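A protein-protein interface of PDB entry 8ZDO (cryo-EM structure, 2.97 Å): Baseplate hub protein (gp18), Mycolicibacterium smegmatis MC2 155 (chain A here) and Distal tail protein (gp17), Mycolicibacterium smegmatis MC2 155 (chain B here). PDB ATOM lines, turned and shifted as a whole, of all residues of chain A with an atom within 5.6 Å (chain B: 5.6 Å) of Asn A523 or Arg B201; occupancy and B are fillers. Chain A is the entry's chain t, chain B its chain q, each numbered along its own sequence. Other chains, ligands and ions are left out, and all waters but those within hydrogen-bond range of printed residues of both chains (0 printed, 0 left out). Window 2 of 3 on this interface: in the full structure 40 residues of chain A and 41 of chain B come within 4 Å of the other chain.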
ATOM      1  N   GLY A 310     -18.747 -10.633   0.432  1.00  0.00           N
ATOM      2  CA  GLY A 310     -17.465 -10.960   1.024  1.00  0.00           C
ATOM      3  C   GLY A 310     -17.646 -11.715   2.319  1.00  0.00           C
ATOM      4  O   GLY A 310     -18.767 -11.964   2.777  1.00  0.00           O
ATOM      5  N   THR A 311     -16.515 -12.078   2.912  1.00  0.00           N
ATOM      6  CA  THR A 311     -16.492 -12.727   4.210  1.00  0.00           C
ATOM      7  C   THR A 311     -15.482 -12.020   5.099  1.00  0.00           C
ATOM      8  O   THR A 311     -14.512 -11.430   4.618  1.00  0.00           O
ATOM      9  CB  THR A 311     -16.145 -14.218   4.107  1.00  0.00           C
ATOM     10  OG1 THR A 311     -14.864 -14.375   3.489  1.00  0.00           O
ATOM     11  CG2 THR A 311     -17.189 -14.959   3.286  1.00  0.00           C
ATOM     12  N   ILE A 312     -15.725 -12.089   6.407  1.00  0.00           N
ATOM     13  CA  ILE A 312     -14.875 -11.405   7.374  1.00  0.00           C
ATOM     14  C   ILE A 312     -13.471 -11.980   7.444  1.00  0.00           C
ATOM     15  O   ILE A 312     -12.596 -11.372   8.070  1.00  0.00           O
ATOM     16  CB  ILE A 312     -15.512 -11.433   8.778  1.00  0.00           C
ATOM     17  CG1 ILE A 312     -15.400 -12.828   9.390  1.00  0.00           C
ATOM     18  CG2 ILE A 312     -16.962 -11.011   8.711  1.00  0.00           C
ATOM     19  CD1 ILE A 312     -15.987 -12.927  10.773  1.00  0.00           C
ATOM     20  N   VAL A 313     -13.227 -13.135   6.821  1.00  0.00           N
ATOM     21  CA  VAL A 313     -11.913 -13.767   6.875  1.00  0.00           C
ATOM     22  C   VAL A 313     -11.092 -13.541   5.613  1.00  0.00           C
ATOM     23  O   VAL A 313      -9.879 -13.805   5.627  1.00  0.00           O
ATOM     24  CB  VAL A 313     -12.033 -15.280   7.153  1.00  0.00           C
ATOM     25  CG1 VAL A 313     -12.726 -15.514   8.483  1.00  0.00           C
ATOM     26  CG2 VAL A 313     -12.783 -15.966   6.030  1.00  0.00           C
ATOM     27  N   THR A 515     -21.861  -6.894   9.074  1.00  0.00           N
ATOM     28  CA  THR A 515     -22.071  -8.238   9.585  1.00  0.00           C
ATOM     29  C   THR A 515     -23.059  -8.201  10.740  1.00  0.00           C
ATOM     30  O   THR A 515     -23.293  -7.158  11.356  1.00  0.00           O
ATOM     31  CB  THR A 515     -20.763  -8.887  10.054  1.00  0.00           C
ATOM     32  OG1 THR A 515     -20.391  -8.348  11.325  1.00  0.00           O
ATOM     33  CG2 THR A 515     -19.656  -8.616   9.061  1.00  0.00           C
ATOM     34  N   GLY A 520     -24.566 -18.881  11.861  1.00  0.00           N
ATOM     35  CA  GLY A 520     -24.730 -19.224  10.471  1.00  0.00           C
ATOM     36  C   GLY A 520     -24.369 -18.120   9.500  1.00  0.00           C
ATOM     37  O   GLY A 520     -24.140 -18.406   8.320  1.00  0.00           O
ATOM     38  N   VAL A 521     -24.312 -16.871   9.957  1.00  0.00           N
ATOM     39  CA  VAL A 521     -23.975 -15.756   9.081  1.00  0.00           C
ATOM     40  C   VAL A 521     -22.898 -14.882   9.710  1.00  0.00           C
ATOM     41  O   VAL A 521     -22.773 -13.702   9.370  1.00  0.00           O
ATOM     42  CB  VAL A 521     -25.221 -14.921   8.742  1.00  0.00           C
ATOM     43  CG1 VAL A 521     -26.154 -15.705   7.841  1.00  0.00           C
ATOM     44  CG2 VAL A 521     -25.935 -14.498  10.010  1.00  0.00           C
ATOM     45  N   GLU A 522     -22.120 -15.446  10.636  1.00  0.00           N
ATOM     46  CA  GLU A 522     -21.032 -14.681  11.237  1.00  0.00           C
ATOM     47  C   GLU A 522     -19.992 -14.297  10.192  1.00  0.00           C
ATOM     48  O   GLU A 522     -19.518 -13.156  10.158  1.00  0.00           O
ATOM     49  CB  GLU A 522     -20.371 -15.479  12.361  1.00  0.00           C
ATOM     50  CG  GLU A 522     -21.198 -15.651  13.615  1.00  0.00           C
ATOM     51  CD  GLU A 522     -21.708 -17.067  13.778  1.00  0.00           C
ATOM     52  OE1 GLU A 522     -21.578 -17.859  12.823  1.00  0.00           O
ATOM     53  OE2 GLU A 522     -22.214 -17.396  14.872  1.00  0.00           O
ATOM     54  N   ASN A 523     -19.627 -15.244   9.328  1.00  0.00           N
ATOM     55  CA  ASN A 523     -18.598 -14.985   8.328  1.00  0.00           C
ATOM     56  C   ASN A 523     -19.109 -14.095   7.204  1.00  0.00           C
ATOM     57  O   ASN A 523     -18.338 -13.313   6.641  1.00  0.00           O
ATOM     58  CB  ASN A 523     -18.082 -16.307   7.764  1.00  0.00           C
ATOM     59  CG  ASN A 523     -16.731 -16.169   7.099  1.00  0.00           C
ATOM     60  OD1 ASN A 523     -15.888 -15.390   7.538  1.00  0.00           O
ATOM     61  ND2 ASN A 523     -16.516 -16.929   6.033  1.00  0.00           N
ATOM     62  N   ILE A 524     -20.397 -14.193   6.875  1.00  0.00           N
ATOM     63  CA  ILE A 524     -20.956 -13.481   5.733  1.00  0.00           C
ATOM     64  C   ILE A 524     -20.899 -11.979   5.969  1.00  0.00           C
ATOM     65  O   ILE A 524     -21.128 -11.496   7.086  1.00  0.00           O
ATOM     66  CB  ILE A 524     -22.401 -13.950   5.484  1.00  0.00           C
ATOM     67  CG1 ILE A 524     -22.422 -15.438   5.147  1.00  0.00           C
ATOM     68  CG2 ILE A 524     -23.049 -13.156   4.369  1.00  0.00           C
ATOM     69  CD1 ILE A 524     -21.662 -15.785   3.896  1.00  0.00           C
ATOM     70  N   VAL A 525     -20.595 -11.226   4.914  1.00  0.00           N
ATOM     71  CA  VAL A 525     -20.655  -9.773   4.927  1.00  0.00           C
ATOM     72  C   VAL A 525     -21.703  -9.357   3.908  1.00  0.00           C
ATOM     73  O   VAL A 525     -21.589  -9.692   2.723  1.00  0.00           O
ATOM     74  CB  VAL A 525     -19.293  -9.141   4.599  1.00  0.00           C
ATOM     75  CG1 VAL A 525     -19.455  -7.669   4.294  1.00  0.00           C
ATOM     76  CG2 VAL A 525     -18.326  -9.336   5.745  1.00  0.00           C
ATOM     77  N   SER B 193      -7.288 -18.038  16.170  1.00  0.00           N
ATOM     78  CA  SER B 193      -8.560 -18.121  16.872  1.00  0.00           C
ATOM     79  C   SER B 193      -8.381 -18.586  18.310  1.00  0.00           C
ATOM     80  O   SER B 193      -9.215 -18.274  19.164  1.00  0.00           O
ATOM     81  CB  SER B 193      -9.507 -19.060  16.131  1.00  0.00           C
ATOM     82  OG  SER B 193      -9.192 -20.412  16.401  1.00  0.00           O
ATOM     83  N   ASN B 196     -11.316 -20.373  19.693  1.00  0.00           N
ATOM     84  CA  ASN B 196     -12.538 -19.662  20.036  1.00  0.00           C
ATOM     85  C   ASN B 196     -13.577 -19.834  18.939  1.00  0.00           C
ATOM     86  O   ASN B 196     -13.266 -19.728  17.749  1.00  0.00           O
ATOM     87  CB  ASN B 196     -12.254 -18.181  20.263  1.00  0.00           C
ATOM     88  CG  ASN B 196     -13.385 -17.488  20.979  1.00  0.00           C
ATOM     89  OD1 ASN B 196     -14.295 -18.134  21.495  1.00  0.00           O
ATOM     90  ND2 ASN B 196     -13.337 -16.171  21.018  1.00  0.00           N
ATOM     91  N   ASP B 197     -14.822 -20.076  19.344  1.00  0.00           N
ATOM     92  CA  ASP B 197     -15.886 -20.464  18.428  1.00  0.00           C
ATOM     93  C   ASP B 197     -16.928 -19.365  18.246  1.00  0.00           C
ATOM     94  O   ASP B 197     -18.104 -19.664  18.014  1.00  0.00           O
ATOM     95  CB  ASP B 197     -16.546 -21.748  18.924  1.00  0.00           C
ATOM     96  CG  ASP B 197     -17.033 -22.628  17.796  1.00  0.00           C
ATOM     97  OD1 ASP B 197     -16.699 -22.338  16.630  1.00  0.00           O
ATOM     98  OD2 ASP B 197     -17.748 -23.615  18.073  1.00  0.00           O
ATOM     99  N   MET B 198     -16.527 -18.095  18.346  1.00  0.00           N
ATOM    100  CA  MET B 198     -17.504 -17.019  18.228  1.00  0.00           C
ATOM    101  C   MET B 198     -18.030 -16.888  16.803  1.00  0.00           C
ATOM    102  O   MET B 198     -19.180 -16.480  16.609  1.00  0.00           O
ATOM    103  CB  MET B 198     -16.908 -15.689  18.694  1.00  0.00           C
ATOM    104  CG  MET B 198     -15.971 -15.027  17.701  1.00  0.00           C
ATOM    105  SD  MET B 198     -15.494 -13.352  18.167  1.00  0.00           S
ATOM    106  CE  MET B 198     -14.223 -13.660  19.376  1.00  0.00           C
ATOM    107  N   TYR B 199     -17.214 -17.219  15.803  1.00  0.00           N
ATOM    108  CA  TYR B 199     -17.616 -17.143  14.405  1.00  0.00           C
ATOM    109  C   TYR B 199     -17.899 -18.510  13.804  1.00  0.00           C
ATOM    110  O   TYR B 199     -18.026 -18.622  12.581  1.00  0.00           O
ATOM    111  CB  TYR B 199     -16.544 -16.434  13.578  1.00  0.00           C
ATOM    112  CG  TYR B 199     -16.211 -15.038  14.042  1.00  0.00           C
ATOM    113  CD1 TYR B 199     -17.196 -14.070  14.162  1.00  0.00           C
ATOM    114  CD2 TYR B 199     -14.907 -14.684  14.348  1.00  0.00           C
ATOM    115  CE1 TYR B 199     -16.891 -12.793  14.583  1.00  0.00           C
ATOM    116  CE2 TYR B 199     -14.595 -13.413  14.770  1.00  0.00           C
ATOM    117  CZ  TYR B 199     -15.588 -12.472  14.884  1.00  0.00           C
ATOM    118  OH  TYR B 199     -15.273 -11.202  15.304  1.00  0.00           O
ATOM    119  N   SER B 200     -17.991 -19.552  14.633  1.00  0.00           N
ATOM    120  CA  SER B 200     -18.130 -20.932  14.169  1.00  0.00           C
ATOM    121  C   SER B 200     -16.968 -21.342  13.270  1.00  0.00           C
ATOM    122  O   SER B 200     -17.142 -22.105  12.318  1.00  0.00           O
ATOM    123  CB  SER B 200     -19.467 -21.155  13.455  1.00  0.00           C
ATOM    124  OG  SER B 200     -20.555 -20.905  14.327  1.00  0.00           O
ATOM    125  N   ARG B 201     -15.775 -20.832  13.564  1.00  0.00           N
ATOM    126  CA  ARG B 201     -14.554 -21.156  12.839  1.00  0.00           C
ATOM    127  C   ARG B 201     -13.419 -21.432  13.810  1.00  0.00           C
ATOM    128  O   ARG B 201     -12.264 -21.080  13.560  1.00  0.00           O
ATOM    129  CB  ARG B 201     -14.168 -20.036  11.874  1.00  0.00           C
ATOM    130  CG  ARG B 201     -15.268 -19.618  10.924  1.00  0.00           C
ATOM    131  CD  ARG B 201     -14.812 -18.490  10.025  1.00  0.00           C
ATOM    132  NE  ARG B 201     -13.602 -18.831   9.289  1.00  0.00           N
ATOM    133  CZ  ARG B 201     -13.587 -19.253   8.032  1.00  0.00           C
ATOM    134  NH1 ARG B 201     -14.705 -19.413   7.345  1.00  0.00           N
ATOM    135  NH2 ARG B 201     -12.421 -19.521   7.453  1.00  0.00           N
ATOM    136  N   GLY B 202     -13.738 -22.075  14.932  1.00  0.00           N
ATOM    137  CA  GLY B 202     -12.784 -22.315  15.996  1.00  0.00           C
ATOM    138  C   GLY B 202     -11.480 -22.942  15.555  1.00  0.00           C
ATOM    139  O   GLY B 202     -10.431 -22.295  15.616  1.00  0.00           O
ATOM    140  N   ARG B 203     -11.524 -24.193  15.106  1.00  0.00           N
ATOM    141  CA  ARG B 203     -10.322 -24.852  14.622  1.00  0.00           C
ATOM    142  C   ARG B 203     -10.082 -24.627  13.138  1.00  0.00           C
ATOM    143  O   ARG B 203      -9.026 -25.018  12.631  1.00  0.00           O
ATOM    144  CB  ARG B 203     -10.378 -26.353  14.917  1.00  0.00           C
ATOM    145  CG  ARG B 203     -11.606 -27.057  14.397  1.00  0.00           C
ATOM    146  CD  ARG B 203     -11.714 -28.427  15.030  1.00  0.00           C
ATOM    147  NE  ARG B 203     -10.511 -29.222  14.811  1.00  0.00           N
ATOM    148  CZ  ARG B 203     -10.502 -30.539  14.667  1.00  0.00           C
ATOM    149  NH1 ARG B 203     -11.616 -31.248  14.730  1.00  0.00           N
ATOM    150  NH2 ARG B 203      -9.346 -31.161  14.455  1.00  0.00           N
ATOM    151  N   GLU B 204     -11.030 -24.014  12.434  1.00  0.00           N
ATOM    152  CA  GLU B 204     -10.774 -23.593  11.063  1.00  0.00           C
ATOM    153  C   GLU B 204      -9.780 -22.440  11.022  1.00  0.00           C
ATOM    154  O   GLU B 204      -8.932 -22.376  10.126  1.00  0.00           O
ATOM    155  CB  GLU B 204     -12.091 -23.214  10.387  1.00  0.00           C
ATOM    156  CG  GLU B 204     -11.987 -22.122   9.342  1.00  0.00           C
ATOM    157  CD  GLU B 204     -11.207 -22.549   8.119  1.00  0.00           C
ATOM    158  OE1 GLU B 204     -11.214 -23.752   7.797  1.00  0.00           O
ATOM    159  OE2 GLU B 204     -10.585 -21.676   7.476  1.00  0.00           O
ATOM    160  N   ASP B 205      -9.854 -21.530  11.995  1.00  0.00           N
ATOM    161  CA  ASP B 205      -8.967 -20.375  12.070  1.00  0.00           C
ATOM    162  C   ASP B 205      -7.864 -20.556  13.104  1.00  0.00           C
ATOM    163  O   ASP B 205      -7.415 -19.575  13.705  1.00  0.00           O
ATOM    164  CB  ASP B 205      -9.767 -19.112  12.378  1.00  0.00           C
ATOM    165  CG  ASP B 205     -10.498 -18.577  11.170  1.00  0.00           C
ATOM    166  OD1 ASP B 205     -10.045 -18.831  10.037  1.00  0.00           O
ATOM    167  OD2 ASP B 205     -11.530 -17.902  11.353  1.00  0.00           O
ATOM    168  N   LEU B 206      -7.421 -21.794  13.331  1.00  0.00           N
ATOM    169  CA  LEU B 206      -6.377 -22.034  14.322  1.00  0.00           C
ATOM    170  C   LEU B 206      -5.073 -21.353  13.930  1.00  0.00           C
ATOM    171  O   LEU B 206      -4.375 -20.795  14.784  1.00  0.00           O
ATOM    172  CB  LEU B 206      -6.162 -23.534  14.506  1.00  0.00           C
ATOM    173  CG  LEU B 206      -6.930 -24.192  15.651  1.00  0.00           C
ATOM    174  CD1 LEU B 206      -6.586 -25.666  15.743  1.00  0.00           C
ATOM    175  CD2 LEU B 206      -6.651 -23.485  16.966  1.00  0.00           C
ATOM    176  N   TYR B 251      -9.878 -11.997  16.200  1.00  0.00           N
ATOM    177  CA  TYR B 251      -9.845 -12.814  17.397  1.00  0.00           C
ATOM    178  C   TYR B 251      -8.979 -12.192  18.481  1.00  0.00           C
ATOM    179  O   TYR B 251      -7.884 -11.699  18.194  1.00  0.00           O
ATOM    180  CB  TYR B 251      -9.312 -14.213  17.079  1.00  0.00           C
ATOM    181  CG  TYR B 251     -10.212 -15.021  16.183  1.00  0.00           C
ATOM    182  CD1 TYR B 251     -11.380 -15.584  16.671  1.00  0.00           C
ATOM    183  CD2 TYR B 251      -9.895 -15.223  14.850  1.00  0.00           C
ATOM    184  CE1 TYR B 251     -12.205 -16.322  15.859  1.00  0.00           C
ATOM    185  CE2 TYR B 251     -10.716 -15.960  14.029  1.00  0.00           C
ATOM    186  CZ  TYR B 251     -11.872 -16.508  14.540  1.00  0.00           C
ATOM    187  OH  TYR B 251     -12.698 -17.245  13.729  1.00  0.00           O
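The guanidinium group of Arg B201 sits close to the side-chain amide nitrogen of Asn A523 (3.3 Å).
The backbone NH (N) of Gly A520 lies within hydrogen-bond range of the side-chain carboxylate (OE1) of Glu A522, at 3.3 Å. The backbone NH (N) of Ile A312 sits at hydrogen-bond distance from the backbone carbonyl oxygen (O) of Asn A523 (2.9 Å). OH of Tyr B251 is in hydrogen-bond range of OD2 of Asp B205, at 2.7 Å. The side-chain carboxylate of Glu B204 is in salt-bridge range of the guanidinium group of Arg B201, at 2.8 Å. The side-chain sulfur of Met B198 sits close to the side-chain hydroxyl of Tyr B199, 3.6 Å away. The backbone NH (N) of Ser B193 is in hydrogen-bond range of the backbone carbonyl oxygen (O) of Asp B205 (2.9 Å).
Ile A312 touches Tyr B199. NE of Arg B201 touches CG1 of Val A313 (3.5 Å). CG1 of Val A313 touches OD2 of Asp B205, at 3.9 Å. Glu A522 touches Met B198 (OE2 to O, 3.6 Å). Glu A522 touches Tyr B199. Glu A522 touches Ser B200 (OE1 to OG, 3.5 Å).
Of the printed residues of chain B, Ile A312 touches Tyr B199 (3.8 Å). Of the printed residues of chain B, Asn A523 touches Arg B201 (3.3 Å). Ile A524 touches none of the printed residues of chain B. Printed residues of chain A within 4 Å of Tyr B199: Ile A312 (3.8 Å) and Glu A522 (3.6 Å). Arg B201 touches just these residues of chain A: Val A313 (3.5 Å) and Asn A523 (3.3 Å). Of the printed residues of chain A, Asp B205 touches Val A313 (3.9 Å). The nearest printed residue of chain A that does not touch Arg B201 is Ile A312 (5.7 Å).
Hydrophobic or aromatic side chains of chain B that line the printed part of chain A: Tyr B199. Along chain B the printed residues that touch a printed residue of chain A span positions 198 to 205. Hydrophobic or aromatic side chains of chain A that line the printed part of chain B: Ile A312 and Val A313. Among the printed residues, 7 pairs touch across the chains.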
